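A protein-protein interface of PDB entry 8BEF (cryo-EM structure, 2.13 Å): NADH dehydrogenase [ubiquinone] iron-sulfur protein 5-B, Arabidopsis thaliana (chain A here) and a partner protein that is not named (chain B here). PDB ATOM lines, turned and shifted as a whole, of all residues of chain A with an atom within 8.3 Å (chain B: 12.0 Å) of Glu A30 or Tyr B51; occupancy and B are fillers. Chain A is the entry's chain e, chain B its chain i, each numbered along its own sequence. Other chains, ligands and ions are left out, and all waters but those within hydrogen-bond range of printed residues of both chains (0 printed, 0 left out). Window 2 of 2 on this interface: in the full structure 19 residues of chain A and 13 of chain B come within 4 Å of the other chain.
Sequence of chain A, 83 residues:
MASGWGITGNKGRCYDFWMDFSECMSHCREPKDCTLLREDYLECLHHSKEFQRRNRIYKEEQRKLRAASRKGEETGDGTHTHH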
ATOM      1  N   CYS A  24      -5.610  35.506 -19.613  1.00  0.00           N
ATOM      2  CA  CYS A  24      -5.040  36.106 -18.409  1.00  0.00           C
ATOM      3  C   CYS A  24      -4.665  35.033 -17.397  1.00  0.00           C
ATOM      4  O   CYS A  24      -3.528  34.986 -16.916  1.00  0.00           O
ATOM      5  CB  CYS A  24      -6.028  37.099 -17.787  1.00  0.00           C
ATOM      6  SG  CYS A  24      -5.504  37.872 -16.209  1.00  0.00           S
ATOM      7  N   MET A  25      -5.610  34.148 -17.075  1.00  0.00           N
ATOM      8  CA  MET A  25      -5.358  33.128 -16.063  1.00  0.00           C
ATOM      9  C   MET A  25      -4.288  32.130 -16.489  1.00  0.00           C
ATOM     10  O   MET A  25      -3.686  31.484 -15.627  1.00  0.00           O
ATOM     11  CB  MET A  25      -6.660  32.397 -15.720  1.00  0.00           C
ATOM     12  CG  MET A  25      -7.590  33.216 -14.830  1.00  0.00           C
ATOM     13  SD  MET A  25      -7.561  32.803 -13.070  1.00  0.00           S
ATOM     14  CE  MET A  25      -7.819  31.032 -13.113  1.00  0.00           C
ATOM     15  N   HIS A  27      -1.347  32.637 -17.445  1.00  0.00           N
ATOM     16  CA  HIS A  27       0.005  33.011 -17.055  1.00  0.00           C
ATOM     17  C   HIS A  27       0.092  33.780 -15.748  1.00  0.00           C
ATOM     18  O   HIS A  27       1.205  33.983 -15.254  1.00  0.00           O
ATOM     19  CB  HIS A  27       0.677  33.832 -18.167  1.00  0.00           C
ATOM     20  CG  HIS A  27      -0.144  34.985 -18.644  1.00  0.00           C
ATOM     21  ND1 HIS A  27      -0.410  36.087 -17.859  1.00  0.00           N
ATOM     22  CD2 HIS A  27      -0.753  35.211 -19.830  1.00  0.00           C
ATOM     23  CE1 HIS A  27      -1.151  36.941 -18.541  1.00  0.00           C
ATOM     24  NE2 HIS A  27      -1.375  36.433 -19.740  1.00  0.00           N
ATOM     25  N   CYS A  28      -1.022  34.216 -15.174  1.00  0.00           N
ATOM     26  CA  CYS A  28      -1.009  34.920 -13.900  1.00  0.00           C
ATOM     27  C   CYS A  28      -1.133  33.900 -12.776  1.00  0.00           C
ATOM     28  O   CYS A  28      -2.159  33.225 -12.655  1.00  0.00           O
ATOM     29  CB  CYS A  28      -2.141  35.944 -13.831  1.00  0.00           C
ATOM     30  SG  CYS A  28      -1.864  37.431 -14.815  1.00  0.00           S
ATOM     31  N   ARG A  29      -0.087  33.791 -11.956  1.00  0.00           N
ATOM     32  CA  ARG A  29      -0.055  32.783 -10.903  1.00  0.00           C
ATOM     33  C   ARG A  29      -1.052  33.055  -9.787  1.00  0.00           C
ATOM     34  O   ARG A  29      -1.312  32.153  -8.985  1.00  0.00           O
ATOM     35  CB  ARG A  29       1.361  32.676 -10.331  1.00  0.00           C
ATOM     36  CG  ARG A  29       2.333  31.936 -11.239  1.00  0.00           C
ATOM     37  CD  ARG A  29       3.675  31.710 -10.562  1.00  0.00           C
ATOM     38  NE  ARG A  29       4.310  32.962 -10.171  1.00  0.00           N
ATOM     39  CZ  ARG A  29       5.014  33.734 -10.988  1.00  0.00           C
ATOM     40  NH1 ARG A  29       5.202  33.408 -12.256  1.00  0.00           N
ATOM     41  NH2 ARG A  29       5.542  34.862 -10.522  1.00  0.00           N
ATOM     42  N   GLU A  30      -1.609  34.262  -9.711  1.00  0.00           N
ATOM     43  CA  GLU A  30      -2.631  34.601  -8.727  1.00  0.00           C
ATOM     44  C   GLU A  30      -3.930  34.951  -9.441  1.00  0.00           C
ATOM     45  O   GLU A  30      -3.947  35.890 -10.256  1.00  0.00           O
ATOM     46  CB  GLU A  30      -2.179  35.766  -7.847  1.00  0.00           C
ATOM     47  CG  GLU A  30      -1.086  35.412  -6.860  1.00  0.00           C
ATOM     48  CD  GLU A  30       0.104  36.345  -6.951  1.00  0.00           C
ATOM     49  OE1 GLU A  30       0.165  37.141  -7.911  1.00  0.00           O
ATOM     50  OE2 GLU A  30       0.981  36.281  -6.064  1.00  0.00           O
ATOM     51  N   PRO A  31      -5.032  34.244  -9.181  1.00  0.00           N
ATOM     52  CA  PRO A  31      -6.290  34.567  -9.872  1.00  0.00           C
ATOM     53  C   PRO A  31      -6.816  35.957  -9.565  1.00  0.00           C
ATOM     54  O   PRO A  31      -7.585  36.498 -10.368  1.00  0.00           O
ATOM     55  CB  PRO A  31      -7.251  33.478  -9.375  1.00  0.00           C
ATOM     56  CG  PRO A  31      -6.695  33.076  -8.050  1.00  0.00           C
ATOM     57  CD  PRO A  31      -5.204  33.160  -8.200  1.00  0.00           C
ATOM     58  N   LYS A  32      -6.421  36.558  -8.441  1.00  0.00           N
ATOM     59  CA  LYS A  32      -6.847  37.917  -8.130  1.00  0.00           C
ATOM     60  C   LYS A  32      -6.362  38.925  -9.163  1.00  0.00           C
ATOM     61  O   LYS A  32      -6.927  40.018  -9.258  1.00  0.00           O
ATOM     62  CB  LYS A  32      -6.353  38.318  -6.740  1.00  0.00           C
ATOM     63  CG  LYS A  32      -7.389  38.144  -5.643  1.00  0.00           C
ATOM     64  CD  LYS A  32      -7.080  39.023  -4.444  1.00  0.00           C
ATOM     65  CE  LYS A  32      -8.253  39.062  -3.478  1.00  0.00           C
ATOM     66  NZ  LYS A  32      -8.287  40.326  -2.693  1.00  0.00           N
ATOM     67  N   ASP A  33      -5.334  38.584  -9.943  1.00  0.00           N
ATOM     68  CA  ASP A  33      -4.899  39.463 -11.020  1.00  0.00           C
ATOM     69  C   ASP A  33      -5.838  39.428 -12.219  1.00  0.00           C
ATOM     70  O   ASP A  33      -5.772  40.323 -13.065  1.00  0.00           O
ATOM     71  CB  ASP A  33      -3.484  39.092 -11.465  1.00  0.00           C
ATOM     72  CG  ASP A  33      -2.421  39.948 -10.799  1.00  0.00           C
ATOM     73  OD1 ASP A  33      -1.442  39.381 -10.275  1.00  0.00           O
ATOM     74  OD2 ASP A  33      -2.568  41.188 -10.799  1.00  0.00           O
ATOM     75  N   CYS A  34      -6.701  38.418 -12.316  1.00  0.00           N
ATOM     76  CA  CYS A  34      -7.647  38.305 -13.419  1.00  0.00           C
ATOM     77  C   CYS A  34      -9.085  38.561 -12.973  1.00  0.00           C
ATOM     78  O   CYS A  34     -10.026  38.174 -13.670  1.00  0.00           O
ATOM     79  CB  CYS A  34      -7.531  36.930 -14.079  1.00  0.00           C
ATOM     80  SG  CYS A  34      -5.882  36.513 -14.739  1.00  0.00           S
ATOM     81  N   THR A  35      -9.266  39.217 -11.823  1.00  0.00           N
ATOM     82  CA  THR A  35     -10.604  39.442 -11.287  1.00  0.00           C
ATOM     83  C   THR A  35     -11.447  40.305 -12.223  1.00  0.00           C
ATOM     84  O   THR A  35     -12.630  40.020 -12.446  1.00  0.00           O
ATOM     85  CB  THR A  35     -10.500  40.087  -9.901  1.00  0.00           C
ATOM     86  OG1 THR A  35     -10.157  39.090  -8.931  1.00  0.00           O
ATOM     87  CG2 THR A  35     -11.811  40.737  -9.500  1.00  0.00           C
ATOM     88  N   ALA B  45       3.824  18.343   3.898  1.00  0.00           N
ATOM     89  CA  ALA B  45       3.426  19.740   3.798  1.00  0.00           C
ATOM     90  C   ALA B  45       3.244  20.207   2.360  1.00  0.00           C
ATOM     91  O   ALA B  45       2.919  21.379   2.143  1.00  0.00           O
ATOM     92  CB  ALA B  45       4.455  20.633   4.500  1.00  0.00           C
ATOM     93  N   LEU B  46       3.444  19.329   1.381  1.00  0.00           N
ATOM     94  CA  LEU B  46       3.284  19.717  -0.016  1.00  0.00           C
ATOM     95  C   LEU B  46       1.822  20.046  -0.296  1.00  0.00           C
ATOM     96  O   LEU B  46       0.935  19.264   0.070  1.00  0.00           O
ATOM     97  CB  LEU B  46       3.758  18.598  -0.943  1.00  0.00           C
ATOM     98  CG  LEU B  46       5.071  18.821  -1.698  1.00  0.00           C
ATOM     99  CD1 LEU B  46       5.541  17.529  -2.343  1.00  0.00           C
ATOM    100  CD2 LEU B  46       4.920  19.912  -2.743  1.00  0.00           C
ATOM    101  N   PRO B  47       1.529  21.182  -0.924  1.00  0.00           N
ATOM    102  CA  PRO B  47       0.128  21.539  -1.181  1.00  0.00           C
ATOM    103  C   PRO B  47      -0.531  20.555  -2.135  1.00  0.00           C
ATOM    104  O   PRO B  47       0.053  20.150  -3.143  1.00  0.00           O
ATOM    105  CB  PRO B  47       0.230  22.941  -1.793  1.00  0.00           C
ATOM    106  CG  PRO B  47       1.592  22.978  -2.394  1.00  0.00           C
ATOM    107  CD  PRO B  47       2.454  22.202  -1.442  1.00  0.00           C
ATOM    108  N   ILE B  48      -1.776  20.180  -1.904  1.00  0.00           N
ATOM    109  CA  ILE B  48      -2.450  19.282  -2.860  1.00  0.00           C
ATOM    110  C   ILE B  48      -2.857  20.127  -4.075  1.00  0.00           C
ATOM    111  O   ILE B  48      -2.910  19.574  -5.198  1.00  0.00           O
ATOM    112  CB  ILE B  48      -3.643  18.623  -2.129  1.00  0.00           C
ATOM    113  CG1 ILE B  48      -4.431  17.630  -2.979  1.00  0.00           C
ATOM    114  CG2 ILE B  48      -4.562  19.692  -1.553  1.00  0.00           C
ATOM    115  CD1 ILE B  48      -5.732  17.232  -2.337  1.00  0.00           C
ATOM    116  N   ARG B  49      -3.156  21.410  -3.832  1.00  0.00           N
ATOM    117  CA  ARG B  49      -3.452  22.300  -4.946  1.00  0.00           C
ATOM    118  C   ARG B  49      -2.222  23.157  -5.204  1.00  0.00           C
ATOM    119  O   ARG B  49      -1.967  24.117  -4.459  1.00  0.00           O
ATOM    120  CB  ARG B  49      -4.669  23.170  -4.616  1.00  0.00           C
ATOM    121  CG  ARG B  49      -5.265  23.945  -5.777  1.00  0.00           C
ATOM    122  CD  ARG B  49      -4.630  25.323  -5.899  1.00  0.00           C
ATOM    123  NE  ARG B  49      -4.859  26.137  -4.711  1.00  0.00           N
ATOM    124  CZ  ARG B  49      -4.355  27.350  -4.527  1.00  0.00           C
ATOM    125  NH1 ARG B  49      -3.592  27.927  -5.441  1.00  0.00           N
ATOM    126  NH2 ARG B  49      -4.627  28.001  -3.400  1.00  0.00           N
ATOM    127  N   PRO B  50      -1.415  22.808  -6.242  1.00  0.00           N
ATOM    128  CA  PRO B  50      -0.193  23.559  -6.469  1.00  0.00           C
ATOM    129  C   PRO B  50      -0.459  25.037  -6.795  1.00  0.00           C
ATOM    130  O   PRO B  50      -1.579  25.376  -7.083  1.00  0.00           O
ATOM    131  CB  PRO B  50       0.454  22.731  -7.603  1.00  0.00           C
ATOM    132  CG  PRO B  50      -0.666  22.121  -8.351  1.00  0.00           C
ATOM    133  CD  PRO B  50      -1.589  21.728  -7.236  1.00  0.00           C
ATOM    134  N   TYR B  51       0.547  25.873  -6.716  1.00  0.00           N
ATOM    135  CA  TYR B  51       0.454  27.282  -7.069  1.00  0.00           C
ATOM    136  C   TYR B  51       0.202  27.440  -8.561  1.00  0.00           C
ATOM    137  O   TYR B  51       1.044  27.066  -9.385  1.00  0.00           O
ATOM    138  CB  TYR B  51       1.745  27.992  -6.666  1.00  0.00           C
ATOM    139  CG  TYR B  51       1.649  29.497  -6.558  1.00  0.00           C
ATOM    140  CD1 TYR B  51       0.575  30.105  -5.926  1.00  0.00           C
ATOM    141  CD2 TYR B  51       2.644  30.309  -7.085  1.00  0.00           C
ATOM    142  CE1 TYR B  51       0.494  31.480  -5.822  1.00  0.00           C
ATOM    143  CE2 TYR B  51       2.573  31.680  -6.986  1.00  0.00           C
ATOM    144  CZ  TYR B  51       1.498  32.262  -6.354  1.00  0.00           C
ATOM    145  OH  TYR B  51       1.431  33.630  -6.259  1.00  0.00           O
ATOM    146  N   GLY B  52      -0.954  28.000  -8.909  1.00  0.00           N
ATOM    147  CA  GLY B  52      -1.282  28.265 -10.295  1.00  0.00           C
ATOM    148  C   GLY B  52      -1.331  27.026 -11.163  1.00  0.00           C
ATOM    149  O   GLY B  52      -0.717  26.994 -12.230  1.00  0.00           O
ATOM    150  N   PHE B  53      -2.043  25.989 -10.712  1.00  0.00           N
ATOM    151  CA  PHE B  53      -2.095  24.753 -11.486  1.00  0.00           C
ATOM    152  C   PHE B  53      -2.730  24.985 -12.852  1.00  0.00           C
ATOM    153  O   PHE B  53      -2.300  24.399 -13.850  1.00  0.00           O
ATOM    154  CB  PHE B  53      -2.852  23.672 -10.716  1.00  0.00           C
ATOM    155  CG  PHE B  53      -4.282  24.020 -10.420  1.00  0.00           C
ATOM    156  CD1 PHE B  53      -4.613  24.764  -9.301  1.00  0.00           C
ATOM    157  CD2 PHE B  53      -5.299  23.595 -11.256  1.00  0.00           C
ATOM    158  CE1 PHE B  53      -5.930  25.080  -9.030  1.00  0.00           C
ATOM    159  CE2 PHE B  53      -6.615  23.911 -10.988  1.00  0.00           C
ATOM    160  CZ  PHE B  53      -6.930  24.651  -9.876  1.00  0.00           C
ATOM    161  N   TRP B  54      -3.734  25.863 -12.922  1.00  0.00           N
ATOM    162  CA  TRP B  54      -4.397  26.168 -14.184  1.00  0.00           C
ATOM    163  C   TRP B  54      -3.465  26.825 -15.195  1.00  0.00           C
ATOM    164  O   TRP B  54      -3.822  26.909 -16.375  1.00  0.00           O
ATOM    165  CB  TRP B  54      -5.613  27.059 -13.927  1.00  0.00           C
ATOM    166  CG  TRP B  54      -5.241  28.358 -13.302  1.00  0.00           C
ATOM    167  CD1 TRP B  54      -4.892  29.499 -13.946  1.00  0.00           C
ATOM    168  CD2 TRP B  54      -5.149  28.642 -11.902  1.00  0.00           C
ATOM    169  NE1 TRP B  54      -4.594  30.486 -13.037  1.00  0.00           N
ATOM    170  CE2 TRP B  54      -4.745  29.983 -11.773  1.00  0.00           C
ATOM    171  CE3 TRP B  54      -5.373  27.892 -10.745  1.00  0.00           C
ATOM    172  CZ2 TRP B  54      -4.566  30.592 -10.535  1.00  0.00           C
ATOM    173  CZ3 TRP B  54      -5.192  28.497  -9.516  1.00  0.00           C
ATOM    174  CH2 TRP B  54      -4.792  29.835  -9.421  1.00  0.00           C
ATOM    175  N   THR B  55      -2.296  27.300 -14.763  1.00  0.00           N
ATOM    176  CA  THR B  55      -1.262  27.770 -15.678  1.00  0.00           C
ATOM    177  C   THR B  55      -0.584  26.632 -16.433  1.00  0.00           C
ATOM    178  O   THR B  55      -0.084  26.853 -17.542  1.00  0.00           O
ATOM    179  CB  THR B  55      -0.220  28.580 -14.897  1.00  0.00           C
ATOM    180  OG1 THR B  55      -0.872  29.643 -14.194  1.00  0.00           O
ATOM    181  CG2 THR B  55       0.847  29.163 -15.813  1.00  0.00           C
ATOM    182  N   PHE B  56      -0.552  25.414 -15.861  1.00  0.00           N
ATOM    183  CA  PHE B  56       0.148  24.251 -16.437  1.00  0.00           C
ATOM    184  C   PHE B  56      -0.440  23.911 -17.826  1.00  0.00           C
ATOM    185  O   PHE B  56      -1.678  23.898 -17.958  1.00  0.00           O
ATOM    186  CB  PHE B  56       0.150  23.106 -15.435  1.00  0.00           C
ATOM    187  CG  PHE B  56       0.663  23.362 -14.041  1.00  0.00           C
ATOM    188  CD1 PHE B  56       1.515  24.414 -13.757  1.00  0.00           C
ATOM    189  CD2 PHE B  56       0.278  22.532 -13.001  1.00  0.00           C
ATOM    190  CE1 PHE B  56       1.959  24.636 -12.465  1.00  0.00           C
ATOM    191  CE2 PHE B  56       0.713  22.763 -11.704  1.00  0.00           C
ATOM    192  CZ  PHE B  56       1.558  23.812 -11.444  1.00  0.00           C
ATOM    193  N   GLU B  57       0.406  23.652 -18.815  1.00  0.00           N
ATOM    194  CA  GLU B  57       0.016  23.544 -20.217  1.00  0.00           C
ATOM    195  C   GLU B  57      -1.120  22.552 -20.427  1.00  0.00           C
ATOM    196  O   GLU B  57      -1.964  22.759 -21.306  1.00  0.00           O
ATOM    197  CB  GLU B  57       1.224  23.148 -21.066  1.00  0.00           C
ATOM    198  CG  GLU B  57       2.160  24.302 -21.384  1.00  0.00           C
ATOM    199  CD  GLU B  57       3.002  24.720 -20.192  1.00  0.00           C
ATOM    200  OE1 GLU B  57       3.113  23.928 -19.233  1.00  0.00           O
ATOM    201  OE2 GLU B  57       3.552  25.841 -20.214  1.00  0.00           O
ATOM    202  N   ARG B  58      -1.160  21.473 -19.639  1.00  0.00           N
ATOM    203  CA  ARG B  58      -2.246  20.507 -19.762  1.00  0.00           C
ATOM    204  C   ARG B  58      -3.609  21.166 -19.574  1.00  0.00           C
ATOM    205  O   ARG B  58      -4.603  20.714 -20.151  1.00  0.00           O
ATOM    206  CB  ARG B  58      -2.055  19.373 -18.752  1.00  0.00           C
ATOM    207  CG  ARG B  58      -3.256  18.451 -18.588  1.00  0.00           C
ATOM    208  CD  ARG B  58      -3.473  17.597 -19.828  1.00  0.00           C
ATOM    209  NE  ARG B  58      -4.351  18.232 -20.804  1.00  0.00           N
ATOM    210  CZ  ARG B  58      -4.565  17.771 -22.029  1.00  0.00           C
ATOM    211  NH1 ARG B  58      -3.986  16.665 -22.463  1.00  0.00           N
ATOM    212  NH2 ARG B  58      -5.382  18.438 -22.840  1.00  0.00           N
ATOM    213  N   HIS B  59      -3.641  22.260 -18.828  1.00  0.00           N
ATOM    214  CA  HIS B  59      -4.930  22.892 -18.506  1.00  0.00           C
ATOM    215  C   HIS B  59      -5.303  24.022 -19.491  1.00  0.00           C
ATOM    216  O   HIS B  59      -6.360  24.591 -19.362  1.00  0.00           O
ATOM    217  CB  HIS B  59      -4.829  23.329 -17.077  1.00  0.00           C
ATOM    218  CG  HIS B  59      -4.379  22.301 -16.087  1.00  0.00           C
ATOM    219  ND1 HIS B  59      -4.284  22.583 -14.749  1.00  0.00           N
ATOM    220  CD2 HIS B  59      -3.980  21.018 -16.221  1.00  0.00           C
ATOM    221  CE1 HIS B  59      -3.849  21.526 -14.100  1.00  0.00           C
ATOM    222  NE2 HIS B  59      -3.649  20.553 -14.981  1.00  0.00           N
ATOM    223  N   ASN B  60      -4.414  24.355 -20.396  1.00  0.00           N
ATOM    224  CA  ASN B  60      -4.657  25.421 -21.361  1.00  0.00           C
ATOM    225  C   ASN B  60      -4.990  24.853 -22.737  1.00  0.00           C
ATOM    226  O   ASN B  60      -4.608  25.410 -23.767  1.00  0.00           O
ATOM    227  CB  ASN B  60      -3.456  26.360 -21.446  1.00  0.00           C
ATOM    228  CG  ASN B  60      -3.282  27.200 -20.194  1.00  0.00           C
ATOM    229  OD1 ASN B  60      -4.233  27.433 -19.448  1.00  0.00           O
ATOM    230  ND2 ASN B  60      -2.057  27.661 -19.959  1.00  0.00           N
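Among the printed residues, merely in contact across the chains: Pro A31 with Trp B54, Met A25 with Thr B55, Cys A28 with Trp B54, Arg A29 with Tyr B51 and Arg A29 with Trp B54.
Arg A29 touches two residues of chain B.
Glu A30 touches just one residue of chain B: Tyr B51 (2.7 Å).
No residue of chain B comes within 4 Å of Cys A34.
Tyr B51 touches two residues of chain A.
No residue of chain A comes within 4 Å of Gly B52.
Of the printed residues of chain A, Trp B54 touches Met A25, Cys A28, Arg A29 and Pro A31.
Of the printed residues of chain A, Thr B55 touches Met A25.
Asn B60 touches none of the printed residues of chain A.
The nearest residue of chain B that does not touch Glu A30 is Trp B54 (4.5 Å).
The nearest residue of chain A that does not touch Tyr B51 is Pro A31 (6.4 Å).
The side-chain hydroxyl (OH) of Tyr B51 lies within hydrogen-bond range of the side-chain carboxylate (OE2) of Glu A30 (2.7 Å).
The backbone carbonyl oxygen of Met A25 lies close to the indole nitrogen of Trp B54 (2.9 Å).
The backbone carbonyl oxygen of Cys A24 sits close to the side-chain sulfur of Cys A28 (3.6 Å).
The backbone carbonyl oxygen of Trp B54 sits close to the side-chain amide oxygen of Asn B60 (3.1 Å).
N of Met A25 lies within hydrogen-bond range of SG of Cys A34 (3.3 Å).
SG of Cys A34 forms a disulfide with SG of Cys A24 (2.0 Å).
The backbone carbonyl oxygen (O) of Thr B55 is in hydrogen-bond range of the side-chain amide nitrogen (ND2) of Asn B60 (3.2 Å).
OG1 of Thr B55 sits close to O of Gly B52.
Hydrophobic or aromatic side chains of chain B that line the printed part of chain A: Tyr B51 and Trp B54.
Hydrophobic or aromatic side chains of chain A within 4 Å of the printed part of chain B: Met A25 and Pro A31.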
